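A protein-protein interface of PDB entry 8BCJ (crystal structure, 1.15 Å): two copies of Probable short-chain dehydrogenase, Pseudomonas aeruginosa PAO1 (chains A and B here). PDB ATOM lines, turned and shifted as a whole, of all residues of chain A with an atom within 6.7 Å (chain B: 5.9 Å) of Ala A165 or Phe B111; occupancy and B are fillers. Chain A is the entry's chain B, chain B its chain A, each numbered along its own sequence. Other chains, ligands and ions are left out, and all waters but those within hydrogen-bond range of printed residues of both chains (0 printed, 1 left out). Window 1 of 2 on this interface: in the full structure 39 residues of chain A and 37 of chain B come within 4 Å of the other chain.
The side-chain hydroxyl of Ser B168 sits at hydrogen-bond distance from the backbone carbonyl oxygen of Ser A148 (2.7 Å).
NE of Arg B106 lies within salt-bridge range of OD2 of Asp B158 (2.8 Å).
O of Phe B111 lies within hydrogen-bond range of N of Thr B116 (2.9 Å).
N of Thr A116 lies within hydrogen-bond range of O of Phe A111 (2.9 Å).
The side-chain carboxylate (OD2) of Asp A167 lies within hydrogen-bond range of the side-chain hydroxyl (OG) of Ser A148 (2.8 Å).
His B108 touches His A108.
Phe A111 touches Val B115.
Phe A119 touches Asp B158.
Ala A160 touches Ser B168.
Ala B165 touches Ala A161 (CA to O, 3.2 Å).
CB of Ala A165 touches CZ of Phe B111, at 3.999 Å.
CA of Ala A165 touches O of Ala B161, 3.2 Å away.
Ala A165 touches Gly B164.
O of Ala B160 touches CB of Ser A168, at 3.4 Å.
CA of Ala B161 touches CB of Ser A168 (3.9 Å).
Of the printed residues of chain B, Phe A111 touches Phe B111 (3.1 Å), Val B115 (3.8 Å) and Ala B165 (3.99 Å).
Printed residues of chain B within 4 Å of Ala A165: Phe B111 (3.999 Å), Ala B161 (3.2 Å), Gly B164 (3.96 Å) and Ala B165 (3.7 Å).
Arg B106 touches none of the printed residues of chain A.
Printed residues of chain A within 4 Å of Leu B107: Thr A116 and Phe A119.
Arg B109 touches none of the printed residues of chain A.
Printed residues of chain A within 4 Å of Phe B111: Phe A111, Val A115 and Ala A165.
Printed residues of chain A within 4 Å of Gly B164: Gly A164 (3.7 Å), Ala A165 (3.96 Å) and Ser A168 (3.2 Å).
The nearest printed residue of chain A that does not touch Phe B111 is Phe A119 (5.1 Å).
Along chain A the printed residues that touch a printed residue of chain B span positions 108 to 168.
Hydrophobic or aromatic side chains of chain B that line the printed part of chain A: Leu B107, His B108, Phe B111, Val B115, Ala B161 and Ala B165.
Among the printed residues, 24 pairs touch across the chains.
His B108 touches its own counterpart, His A108.
His A108 touches Thr B116, but with the chains exchanged Thr A116 does not touch His B108 (5.3 Å).
Phe A111 touches its own counterpart, Phe B111.
Gly A164 touches Ala B165, and with the chains exchanged Ala A165 touches Gly B164.
Positions printed for both chains: 108, 111, 115, 116, 160, 161, 162, 164, 165 and 168.
Of the 24 pairs that touch across the chains among the printed residues, 18 have their exchanged pair printed and touching as well.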
ATOM      1  N   HIS A 108      -5.917  21.658  -7.194  1.00  0.00           N
ATOM      2  CA  HIS A 108      -6.927  21.996  -8.184  1.00  0.00           C
ATOM      3  C   HIS A 108      -8.045  22.823  -7.566  1.00  0.00           C
ATOM      4  O   HIS A 108      -8.483  23.811  -8.153  1.00  0.00           O
ATOM      5  CB  HIS A 108      -7.451  20.727  -8.852  1.00  0.00           C
ATOM      6  CG  HIS A 108      -6.407  19.989  -9.639  1.00  0.00           C
ATOM      7  ND1 HIS A 108      -6.582  18.697 -10.083  1.00  0.00           N
ATOM      8  CD2 HIS A 108      -5.182  20.369 -10.066  1.00  0.00           C
ATOM      9  CE1 HIS A 108      -5.506  18.311 -10.747  1.00  0.00           C
ATOM     10  NE2 HIS A 108      -4.639  19.305 -10.747  1.00  0.00           N
ATOM     11  N   PHE A 111      -6.623  26.463  -6.658  1.00  0.00           N
ATOM     12  CA  PHE A 111      -6.406  27.278  -7.849  1.00  0.00           C
ATOM     13  C   PHE A 111      -7.698  27.559  -8.590  1.00  0.00           C
ATOM     14  O   PHE A 111      -7.854  28.639  -9.169  1.00  0.00           O
ATOM     15  CB  PHE A 111      -5.333  26.653  -8.734  1.00  0.00           C
ATOM     16  CG  PHE A 111      -3.979  27.098  -8.354  1.00  0.00           C
ATOM     17  CD1 PHE A 111      -3.418  26.670  -7.172  1.00  0.00           C
ATOM     18  CD2 PHE A 111      -3.295  28.012  -9.122  1.00  0.00           C
ATOM     19  CE1 PHE A 111      -2.176  27.137  -6.784  1.00  0.00           C
ATOM     20  CE2 PHE A 111      -2.049  28.472  -8.725  1.00  0.00           C
ATOM     21  CZ  PHE A 111      -1.503  28.038  -7.569  1.00  0.00           C
ATOM     22  N   VAL A 115      -7.705  31.419  -8.531  1.00  0.00           N
ATOM     23  CA  VAL A 115      -7.024  31.852  -9.750  1.00  0.00           C
ATOM     24  C   VAL A 115      -7.954  31.773 -10.949  1.00  0.00           C
ATOM     25  O   VAL A 115      -8.243  32.786 -11.579  1.00  0.00           O
ATOM     26  CB  VAL A 115      -5.725  31.065  -9.993  1.00  0.00           C
ATOM     27  CG1 VAL A 115      -4.987  31.659 -11.186  1.00  0.00           C
ATOM     28  CG2 VAL A 115      -4.828  31.112  -8.749  1.00  0.00           C
ATOM     29  N   THR A 116      -8.423  30.576 -11.270  1.00  0.00           N
ATOM     30  CA  THR A 116      -9.323  30.436 -12.415  1.00  0.00           C
ATOM     31  C   THR A 116     -10.528  31.347 -12.274  1.00  0.00           C
ATOM     32  O   THR A 116     -10.904  32.020 -13.234  1.00  0.00           O
ATOM     33  CB  THR A 116      -9.689  28.978 -12.632  1.00  0.00           C
ATOM     34  OG1 THR A 116      -8.467  28.296 -12.921  1.00  0.00           O
ATOM     35  CG2 THR A 116     -10.653  28.770 -13.775  1.00  0.00           C
ATOM     36  N   PHE A 119      -9.507  34.874 -13.197  1.00  0.00           N
ATOM     37  CA  PHE A 119      -9.327  34.965 -14.648  1.00  0.00           C
ATOM     38  C   PHE A 119     -10.669  35.005 -15.361  1.00  0.00           C
ATOM     39  O   PHE A 119     -10.872  35.824 -16.257  1.00  0.00           O
ATOM     40  CB  PHE A 119      -8.529  33.766 -15.171  1.00  0.00           C
ATOM     41  CG  PHE A 119      -7.036  33.975 -15.225  1.00  0.00           C
ATOM     42  CD1 PHE A 119      -6.248  33.890 -14.100  1.00  0.00           C
ATOM     43  CD2 PHE A 119      -6.417  34.220 -16.441  1.00  0.00           C
ATOM     44  CE1 PHE A 119      -4.868  34.061 -14.183  1.00  0.00           C
ATOM     45  CE2 PHE A 119      -5.043  34.372 -16.533  1.00  0.00           C
ATOM     46  CZ  PHE A 119      -4.274  34.312 -15.403  1.00  0.00           C
ATOM     47  N   SER A 148       1.170  36.066  -0.803  1.00  0.00           N
ATOM     48  CA  SER A 148       1.960  35.964  -2.031  1.00  0.00           C
ATOM     49  C   SER A 148       3.418  36.342  -1.799  1.00  0.00           C
ATOM     50  O   SER A 148       4.308  35.876  -2.520  1.00  0.00           O
ATOM     51  CB  SER A 148       1.375  36.847  -3.124  1.00  0.00           C
ATOM     52  OG  SER A 148       1.641  38.202  -2.815  1.00  0.00           O
ATOM     53  N   ALA A 160      -0.732  30.561  -0.999  1.00  0.00           N
ATOM     54  CA  ALA A 160       0.256  31.592  -1.296  1.00  0.00           C
ATOM     55  C   ALA A 160       0.590  31.618  -2.780  1.00  0.00           C
ATOM     56  O   ALA A 160       0.687  32.691  -3.391  1.00  0.00           O
ATOM     57  CB  ALA A 160       1.522  31.341  -0.480  1.00  0.00           C
ATOM     58  N   ALA A 161       0.792  30.440  -3.369  1.00  0.00           N
ATOM     59  CA  ALA A 161       1.054  30.347  -4.800  1.00  0.00           C
ATOM     60  C   ALA A 161      -0.114  30.881  -5.616  1.00  0.00           C
ATOM     61  O   ALA A 161       0.090  31.603  -6.596  1.00  0.00           O
ATOM     62  CB  ALA A 161       1.381  28.902  -5.168  1.00  0.00           C
ATOM     63  N   ALA A 162      -1.347  30.544  -5.231  1.00  0.00           N
ATOM     64  CA  ALA A 162      -2.514  31.098  -5.924  1.00  0.00           C
ATOM     65  C   ALA A 162      -2.498  32.621  -5.915  1.00  0.00           C
ATOM     66  O   ALA A 162      -2.818  33.247  -6.918  1.00  0.00           O
ATOM     67  CB  ALA A 162      -3.793  30.550  -5.292  1.00  0.00           C
ATOM     68  N   LYS A 163      -2.146  33.221  -4.781  1.00  0.00           N
ATOM     69  CA  LYS A 163      -2.119  34.680  -4.690  1.00  0.00           C
ATOM     70  C   LYS A 163      -0.932  35.265  -5.449  1.00  0.00           C
ATOM     71  O   LYS A 163      -1.053  36.349  -6.017  1.00  0.00           O
ATOM     72  CB  LYS A 163      -2.231  35.091  -3.228  1.00  0.00           C
ATOM     73  CG  LYS A 163      -3.536  34.642  -2.576  1.00  0.00           C
ATOM     74  CD  LYS A 163      -4.771  35.247  -3.230  1.00  0.00           C
ATOM     75  CE  LYS A 163      -6.018  35.070  -2.366  1.00  0.00           C
ATOM     76  NZ  LYS A 163      -7.196  35.760  -2.960  1.00  0.00           N
ATOM     77  N   GLY A 164       0.201  34.562  -5.508  1.00  0.00           N
ATOM     78  CA  GLY A 164       1.263  34.980  -6.410  1.00  0.00           C
ATOM     79  C   GLY A 164       0.822  35.011  -7.859  1.00  0.00           C
ATOM     80  O   GLY A 164       1.216  35.894  -8.620  1.00  0.00           O
ATOM     81  N   ALA A 165       0.002  34.040  -8.262  1.00  0.00           N
ATOM     82  CA  ALA A 165      -0.575  34.039  -9.605  1.00  0.00           C
ATOM     83  C   ALA A 165      -1.436  35.276  -9.827  1.00  0.00           C
ATOM     84  O   ALA A 165      -1.387  35.893 -10.895  1.00  0.00           O
ATOM     85  CB  ALA A 165      -1.393  32.760  -9.814  1.00  0.00           C
ATOM     86  N   ILE A 166      -2.251  35.642  -8.829  1.00  0.00           N
ATOM     87  CA  ILE A 166      -3.048  36.855  -8.920  1.00  0.00           C
ATOM     88  C   ILE A 166      -2.164  38.076  -9.095  1.00  0.00           C
ATOM     89  O   ILE A 166      -2.500  38.972  -9.874  1.00  0.00           O
ATOM     90  CB  ILE A 166      -3.950  36.991  -7.683  1.00  0.00           C
ATOM     91  CG1 ILE A 166      -5.027  35.902  -7.669  1.00  0.00           C
ATOM     92  CG2 ILE A 166      -4.583  38.384  -7.622  1.00  0.00           C
ATOM     93  CD1 ILE A 166      -5.926  35.862  -8.867  1.00  0.00           C
ATOM     94  N   ASP A 167      -1.038  38.153  -8.380  1.00  0.00           N
ATOM     95  CA  ASP A 167      -0.197  39.333  -8.529  1.00  0.00           C
ATOM     96  C   ASP A 167       0.297  39.461  -9.965  1.00  0.00           C
ATOM     97  O   ASP A 167       0.280  40.551 -10.543  1.00  0.00           O
ATOM     98  CB  ASP A 167       0.979  39.285  -7.556  1.00  0.00           C
ATOM     99  CG  ASP A 167       0.566  39.523  -6.111  1.00  0.00           C
ATOM    100  OD1 ASP A 167      -0.626  39.701  -5.851  1.00  0.00           O
ATOM    101  OD2 ASP A 167       1.486  39.549  -5.256  1.00  0.00           O
ATOM    102  N   SER A 168       0.764  38.357 -10.552  1.00  0.00           N
ATOM    103  CA  SER A 168       1.257  38.398 -11.923  1.00  0.00           C
ATOM    104  C   SER A 168       0.134  38.664 -12.914  1.00  0.00           C
ATOM    105  O   SER A 168       0.340  39.387 -13.893  1.00  0.00           O
ATOM    106  CB  SER A 168       1.968  37.091 -12.255  1.00  0.00           C
ATOM    107  OG  SER A 168       3.152  36.926 -11.475  1.00  0.00           O
ATOM    108  N   MET A 169      -1.057  38.104 -12.693  1.00  0.00           N
ATOM    109  CA  MET A 169      -2.187  38.427 -13.567  1.00  0.00           C
ATOM    110  C   MET A 169      -2.547  39.907 -13.489  1.00  0.00           C
ATOM    111  O   MET A 169      -2.916  40.513 -14.498  1.00  0.00           O
ATOM    112  CB  MET A 169      -3.386  37.541 -13.232  1.00  0.00           C
ATOM    113  CG  MET A 169      -4.619  37.779 -14.135  1.00  0.00           C
ATOM    114  SD  MET A 169      -5.812  38.993 -13.533  1.00  0.00           S
ATOM    115  CE  MET A 169      -6.733  37.997 -12.367  1.00  0.00           C
ATOM    116  N   THR A 170      -2.438  40.508 -12.301  1.00  0.00           N
ATOM    117  CA  THR A 170      -2.748  41.927 -12.142  1.00  0.00           C
ATOM    118  C   THR A 170      -1.830  42.760 -13.015  1.00  0.00           C
ATOM    119  O   THR A 170      -2.272  43.650 -13.745  1.00  0.00           O
ATOM    120  CB  THR A 170      -2.603  42.331 -10.672  1.00  0.00           C
ATOM    121  OG1 THR A 170      -3.518  41.597  -9.864  1.00  0.00           O
ATOM    122  CG2 THR A 170      -2.912  43.802 -10.472  1.00  0.00           C
ATOM    123  N   ARG B 106      -7.936  25.743 -20.771  1.00  0.00           N
ATOM    124  CA  ARG B 106      -6.551  26.162 -20.948  1.00  0.00           C
ATOM    125  C   ARG B 106      -5.889  26.467 -19.612  1.00  0.00           C
ATOM    126  O   ARG B 106      -4.754  26.042 -19.367  1.00  0.00           O
ATOM    127  CB  ARG B 106      -6.480  27.372 -21.866  1.00  0.00           C
ATOM    128  CG  ARG B 106      -5.121  27.999 -21.912  1.00  0.00           C
ATOM    129  CD  ARG B 106      -5.017  28.978 -23.065  1.00  0.00           C
ATOM    130  NE  ARG B 106      -3.772  29.721 -22.988  1.00  0.00           N
ATOM    131  CZ  ARG B 106      -3.168  30.283 -24.022  1.00  0.00           C
ATOM    132  NH1 ARG B 106      -3.640  30.168 -25.246  1.00  0.00           N
ATOM    133  NH2 ARG B 106      -2.038  30.947 -23.824  1.00  0.00           N
ATOM    134  N   LEU B 107      -6.579  27.212 -18.739  1.00  0.00           N
ATOM    135  CA  LEU B 107      -6.020  27.497 -17.422  1.00  0.00           C
ATOM    136  C   LEU B 107      -5.679  26.209 -16.691  1.00  0.00           C
ATOM    137  O   LEU B 107      -4.605  26.098 -16.091  1.00  0.00           O
ATOM    138  CB  LEU B 107      -7.002  28.337 -16.612  1.00  0.00           C
ATOM    139  CG  LEU B 107      -7.025  29.803 -17.049  1.00  0.00           C
ATOM    140  CD1 LEU B 107      -8.333  30.491 -16.668  1.00  0.00           C
ATOM    141  CD2 LEU B 107      -5.832  30.558 -16.472  1.00  0.00           C
ATOM    142  N   HIS B 108      -6.568  25.222 -16.737  1.00  0.00           N
ATOM    143  CA  HIS B 108      -6.267  23.971 -16.056  1.00  0.00           C
ATOM    144  C   HIS B 108      -5.004  23.339 -16.619  1.00  0.00           C
ATOM    145  O   HIS B 108      -4.126  22.915 -15.864  1.00  0.00           O
ATOM    146  CB  HIS B 108      -7.424  22.989 -16.112  1.00  0.00           C
ATOM    147  CG  HIS B 108      -7.099  21.689 -15.449  1.00  0.00           C
ATOM    148  ND1 HIS B 108      -7.203  21.504 -14.090  1.00  0.00           N
ATOM    149  CD2 HIS B 108      -6.595  20.536 -15.949  1.00  0.00           C
ATOM    150  CE1 HIS B 108      -6.822  20.277 -13.784  1.00  0.00           C
ATOM    151  NE2 HIS B 108      -6.437  19.672 -14.892  1.00  0.00           N
ATOM    152  N   ARG B 109      -4.886  23.269 -17.949  1.00  0.00           N
ATOM    153  CA  ARG B 109      -3.719  22.594 -18.522  1.00  0.00           C
ATOM    154  C   ARG B 109      -2.435  23.325 -18.143  1.00  0.00           C
ATOM    155  O   ARG B 109      -1.417  22.706 -17.809  1.00  0.00           O
ATOM    156  CB  ARG B 109      -3.814  22.531 -20.041  1.00  0.00           C
ATOM    157  CG  ARG B 109      -4.867  21.588 -20.584  1.00  0.00           C
ATOM    158  CD  ARG B 109      -4.827  21.470 -22.092  1.00  0.00           C
ATOM    159  NE  ARG B 109      -5.060  22.746 -22.772  1.00  0.00           N
ATOM    160  CZ  ARG B 109      -6.231  23.155 -23.242  1.00  0.00           C
ATOM    161  NH1 ARG B 109      -7.340  22.452 -23.061  1.00  0.00           N
ATOM    162  NH2 ARG B 109      -6.288  24.303 -23.909  1.00  0.00           N
ATOM    163  N   VAL B 110      -2.449  24.658 -18.235  1.00  0.00           N
ATOM    164  CA  VAL B 110      -1.240  25.443 -18.005  1.00  0.00           C
ATOM    165  C   VAL B 110      -0.842  25.397 -16.542  1.00  0.00           C
ATOM    166  O   VAL B 110       0.333  25.235 -16.216  1.00  0.00           O
ATOM    167  CB  VAL B 110      -1.454  26.869 -18.550  1.00  0.00           C
ATOM    168  CG1 VAL B 110      -0.363  27.836 -18.101  1.00  0.00           C
ATOM    169  CG2 VAL B 110      -1.568  26.813 -20.083  1.00  0.00           C
ATOM    170  N   PHE B 111      -1.807  25.522 -15.640  1.00  0.00           N
ATOM    171  CA  PHE B 111      -1.480  25.378 -14.228  1.00  0.00           C
ATOM    172  C   PHE B 111      -1.102  23.954 -13.873  1.00  0.00           C
ATOM    173  O   PHE B 111      -0.234  23.744 -13.015  1.00  0.00           O
ATOM    174  CB  PHE B 111      -2.601  25.927 -13.357  1.00  0.00           C
ATOM    175  CG  PHE B 111      -2.438  27.381 -13.108  1.00  0.00           C
ATOM    176  CD1 PHE B 111      -2.639  28.288 -14.133  1.00  0.00           C
ATOM    177  CD2 PHE B 111      -1.983  27.842 -11.903  1.00  0.00           C
ATOM    178  CE1 PHE B 111      -2.414  29.642 -13.936  1.00  0.00           C
ATOM    179  CE2 PHE B 111      -1.772  29.200 -11.706  1.00  0.00           C
ATOM    180  CZ  PHE B 111      -1.976  30.083 -12.727  1.00  0.00           C
ATOM    181  N   ALA B 112      -1.694  22.956 -14.534  1.00  0.00           N
ATOM    182  CA  ALA B 112      -1.387  21.578 -14.188  1.00  0.00           C
ATOM    183  C   ALA B 112       0.080  21.259 -14.420  1.00  0.00           C
ATOM    184  O   ALA B 112       0.725  20.653 -13.560  1.00  0.00           O
ATOM    185  CB  ALA B 112      -2.270  20.618 -14.979  1.00  0.00           C
ATOM    186  N   THR B 113       0.617  21.617 -15.594  1.00  0.00           N
ATOM    187  CA  THR B 113       2.018  21.318 -15.859  1.00  0.00           C
ATOM    188  C   THR B 113       2.938  22.215 -15.059  1.00  0.00           C
ATOM    189  O   THR B 113       3.850  21.730 -14.387  1.00  0.00           O
ATOM    190  CB  THR B 113       2.338  21.458 -17.339  1.00  0.00           C
ATOM    191  OG1 THR B 113       1.648  20.432 -18.063  1.00  0.00           O
ATOM    192  CG2 THR B 113       3.833  21.326 -17.613  1.00  0.00           C
ATOM    193  N   ASN B 114       2.727  23.536 -15.124  1.00  0.00           N
ATOM    194  CA  ASN B 114       3.706  24.471 -14.584  1.00  0.00           C
ATOM    195  C   ASN B 114       3.642  24.572 -13.078  1.00  0.00           C
ATOM    196  O   ASN B 114       4.691  24.753 -12.443  1.00  0.00           O
ATOM    197  CB  ASN B 114       3.484  25.865 -15.186  1.00  0.00           C
ATOM    198  CG  ASN B 114       3.811  25.909 -16.658  1.00  0.00           C
ATOM    199  OD1 ASN B 114       4.987  25.830 -17.052  1.00  0.00           O
ATOM    200  ND2 ASN B 114       2.792  26.029 -17.482  1.00  0.00           N
ATOM    201  N   VAL B 115       2.458  24.493 -12.490  1.00  0.00           N
ATOM    202  CA  VAL B 115       2.314  24.734 -11.061  1.00  0.00           C
ATOM    203  C   VAL B 115       2.112  23.422 -10.325  1.00  0.00           C
ATOM    204  O   VAL B 115       2.936  23.049  -9.488  1.00  0.00           O
ATOM    205  CB  VAL B 115       1.198  25.749 -10.746  1.00  0.00           C
ATOM    206  CG1 VAL B 115       1.193  26.038  -9.243  1.00  0.00           C
ATOM    207  CG2 VAL B 115       1.378  27.027 -11.543  1.00  0.00           C
ATOM    208  N   THR B 116       1.025  22.710 -10.630  1.00  0.00           N
ATOM    209  CA  THR B 116       0.797  21.440  -9.951  1.00  0.00           C
ATOM    210  C   THR B 116       1.981  20.503 -10.113  1.00  0.00           C
ATOM    211  O   THR B 116       2.417  19.889  -9.140  1.00  0.00           O
ATOM    212  CB  THR B 116      -0.515  20.825 -10.419  1.00  0.00           C
ATOM    213  OG1 THR B 116      -1.562  21.735 -10.077  1.00  0.00           O
ATOM    214  CG2 THR B 116      -0.749  19.499  -9.738  1.00  0.00           C
ATOM    215  N   GLY B 117       2.553  20.419 -11.307  1.00  0.00           N
ATOM    216  CA  GLY B 117       3.675  19.514 -11.502  1.00  0.00           C
ATOM    217  C   GLY B 117       4.859  19.854 -10.619  1.00  0.00           C
ATOM    218  O   GLY B 117       5.530  18.968 -10.086  1.00  0.00           O
ATOM    219  N   ASP B 158      -1.941  33.741 -18.602  1.00  0.00           N
ATOM    220  CA  ASP B 158      -2.084  32.493 -17.854  1.00  0.00           C
ATOM    221  C   ASP B 158      -0.734  31.912 -17.426  1.00  0.00           C
ATOM    222  O   ASP B 158      -0.557  31.489 -16.276  1.00  0.00           O
ATOM    223  CB  ASP B 158      -2.871  31.452 -18.665  1.00  0.00           C
ATOM    224  CG  ASP B 158      -2.311  31.176 -20.061  1.00  0.00           C
ATOM    225  OD1 ASP B 158      -1.753  32.056 -20.736  1.00  0.00           O
ATOM    226  OD2 ASP B 158      -2.462  30.018 -20.513  1.00  0.00           O
ATOM    227  N   TYR B 159       0.201  31.843 -18.363  1.00  0.00           N
ATOM    228  CA  TYR B 159       1.551  31.373 -18.071  1.00  0.00           C
ATOM    229  C   TYR B 159       2.277  32.303 -17.107  1.00  0.00           C
ATOM    230  O   TYR B 159       2.948  31.840 -16.180  1.00  0.00           O
ATOM    231  CB  TYR B 159       2.291  31.212 -19.382  1.00  0.00           C
ATOM    232  CG  TYR B 159       3.761  30.937 -19.286  1.00  0.00           C
ATOM    233  CD1 TYR B 159       4.252  29.637 -19.225  1.00  0.00           C
ATOM    234  CD2 TYR B 159       4.664  31.974 -19.324  1.00  0.00           C
ATOM    235  CE1 TYR B 159       5.616  29.400 -19.208  1.00  0.00           C
ATOM    236  CE2 TYR B 159       6.021  31.752 -19.296  1.00  0.00           C
ATOM    237  CZ  TYR B 159       6.489  30.447 -19.264  1.00  0.00           C
ATOM    238  OH  TYR B 159       7.846  30.195 -19.271  1.00  0.00           O
ATOM    239  N   ALA B 160       2.143  33.615 -17.282  1.00  0.00           N
ATOM    240  CA  ALA B 160       2.768  34.549 -16.353  1.00  0.00           C
ATOM    241  C   ALA B 160       2.253  34.320 -14.948  1.00  0.00           C
ATOM    242  O   ALA B 160       3.034  34.315 -13.991  1.00  0.00           O
ATOM    243  CB  ALA B 160       2.507  35.984 -16.779  1.00  0.00           C
ATOM    244  N   ALA B 161       0.947  34.097 -14.806  1.00  0.00           N
ATOM    245  CA  ALA B 161       0.369  33.803 -13.503  1.00  0.00           C
ATOM    246  C   ALA B 161       0.917  32.495 -12.935  1.00  0.00           C
ATOM    247  O   ALA B 161       1.217  32.410 -11.743  1.00  0.00           O
ATOM    248  CB  ALA B 161      -1.156  33.767 -13.636  1.00  0.00           C
ATOM    249  N   ALA B 162       1.026  31.456 -13.766  1.00  0.00           N
ATOM    250  CA  ALA B 162       1.621  30.201 -13.309  1.00  0.00           C
ATOM    251  C   ALA B 162       3.014  30.430 -12.744  1.00  0.00           C
ATOM    252  O   ALA B 162       3.375  29.870 -11.707  1.00  0.00           O
ATOM    253  CB  ALA B 162       1.668  29.202 -14.466  1.00  0.00           C
ATOM    254  N   GLY B 164       4.205  33.351 -11.539  1.00  0.00           N
ATOM    255  CA  GLY B 164       4.040  34.051 -10.276  1.00  0.00           C
ATOM    256  C   GLY B 164       3.747  33.103  -9.129  1.00  0.00           C
ATOM    257  O   GLY B 164       4.218  33.298  -7.999  1.00  0.00           O
ATOM    258  N   ALA B 165       2.957  32.054  -9.401  1.00  0.00           N
ATOM    259  CA  ALA B 165       2.694  31.034  -8.403  1.00  0.00           C
ATOM    260  C   ALA B 165       3.982  30.327  -8.000  1.00  0.00           C
ATOM    261  O   ALA B 165       4.201  30.052  -6.815  1.00  0.00           O
ATOM    262  CB  ALA B 165       1.671  30.031  -8.945  1.00  0.00           C
ATOM    263  N   SER B 168       6.010  32.483  -5.524  1.00  0.00           N
ATOM    264  CA  SER B 168       5.507  32.427  -4.156  1.00  0.00           C
ATOM    265  C   SER B 168       5.738  31.063  -3.524  1.00  0.00           C
ATOM    266  O   SER B 168       6.039  30.972  -2.328  1.00  0.00           O
ATOM    267  CB  SER B 168       4.021  32.789  -4.114  1.00  0.00           C
ATOM    268  OG  SER B 168       3.807  34.141  -4.529  1.00  0.00           O
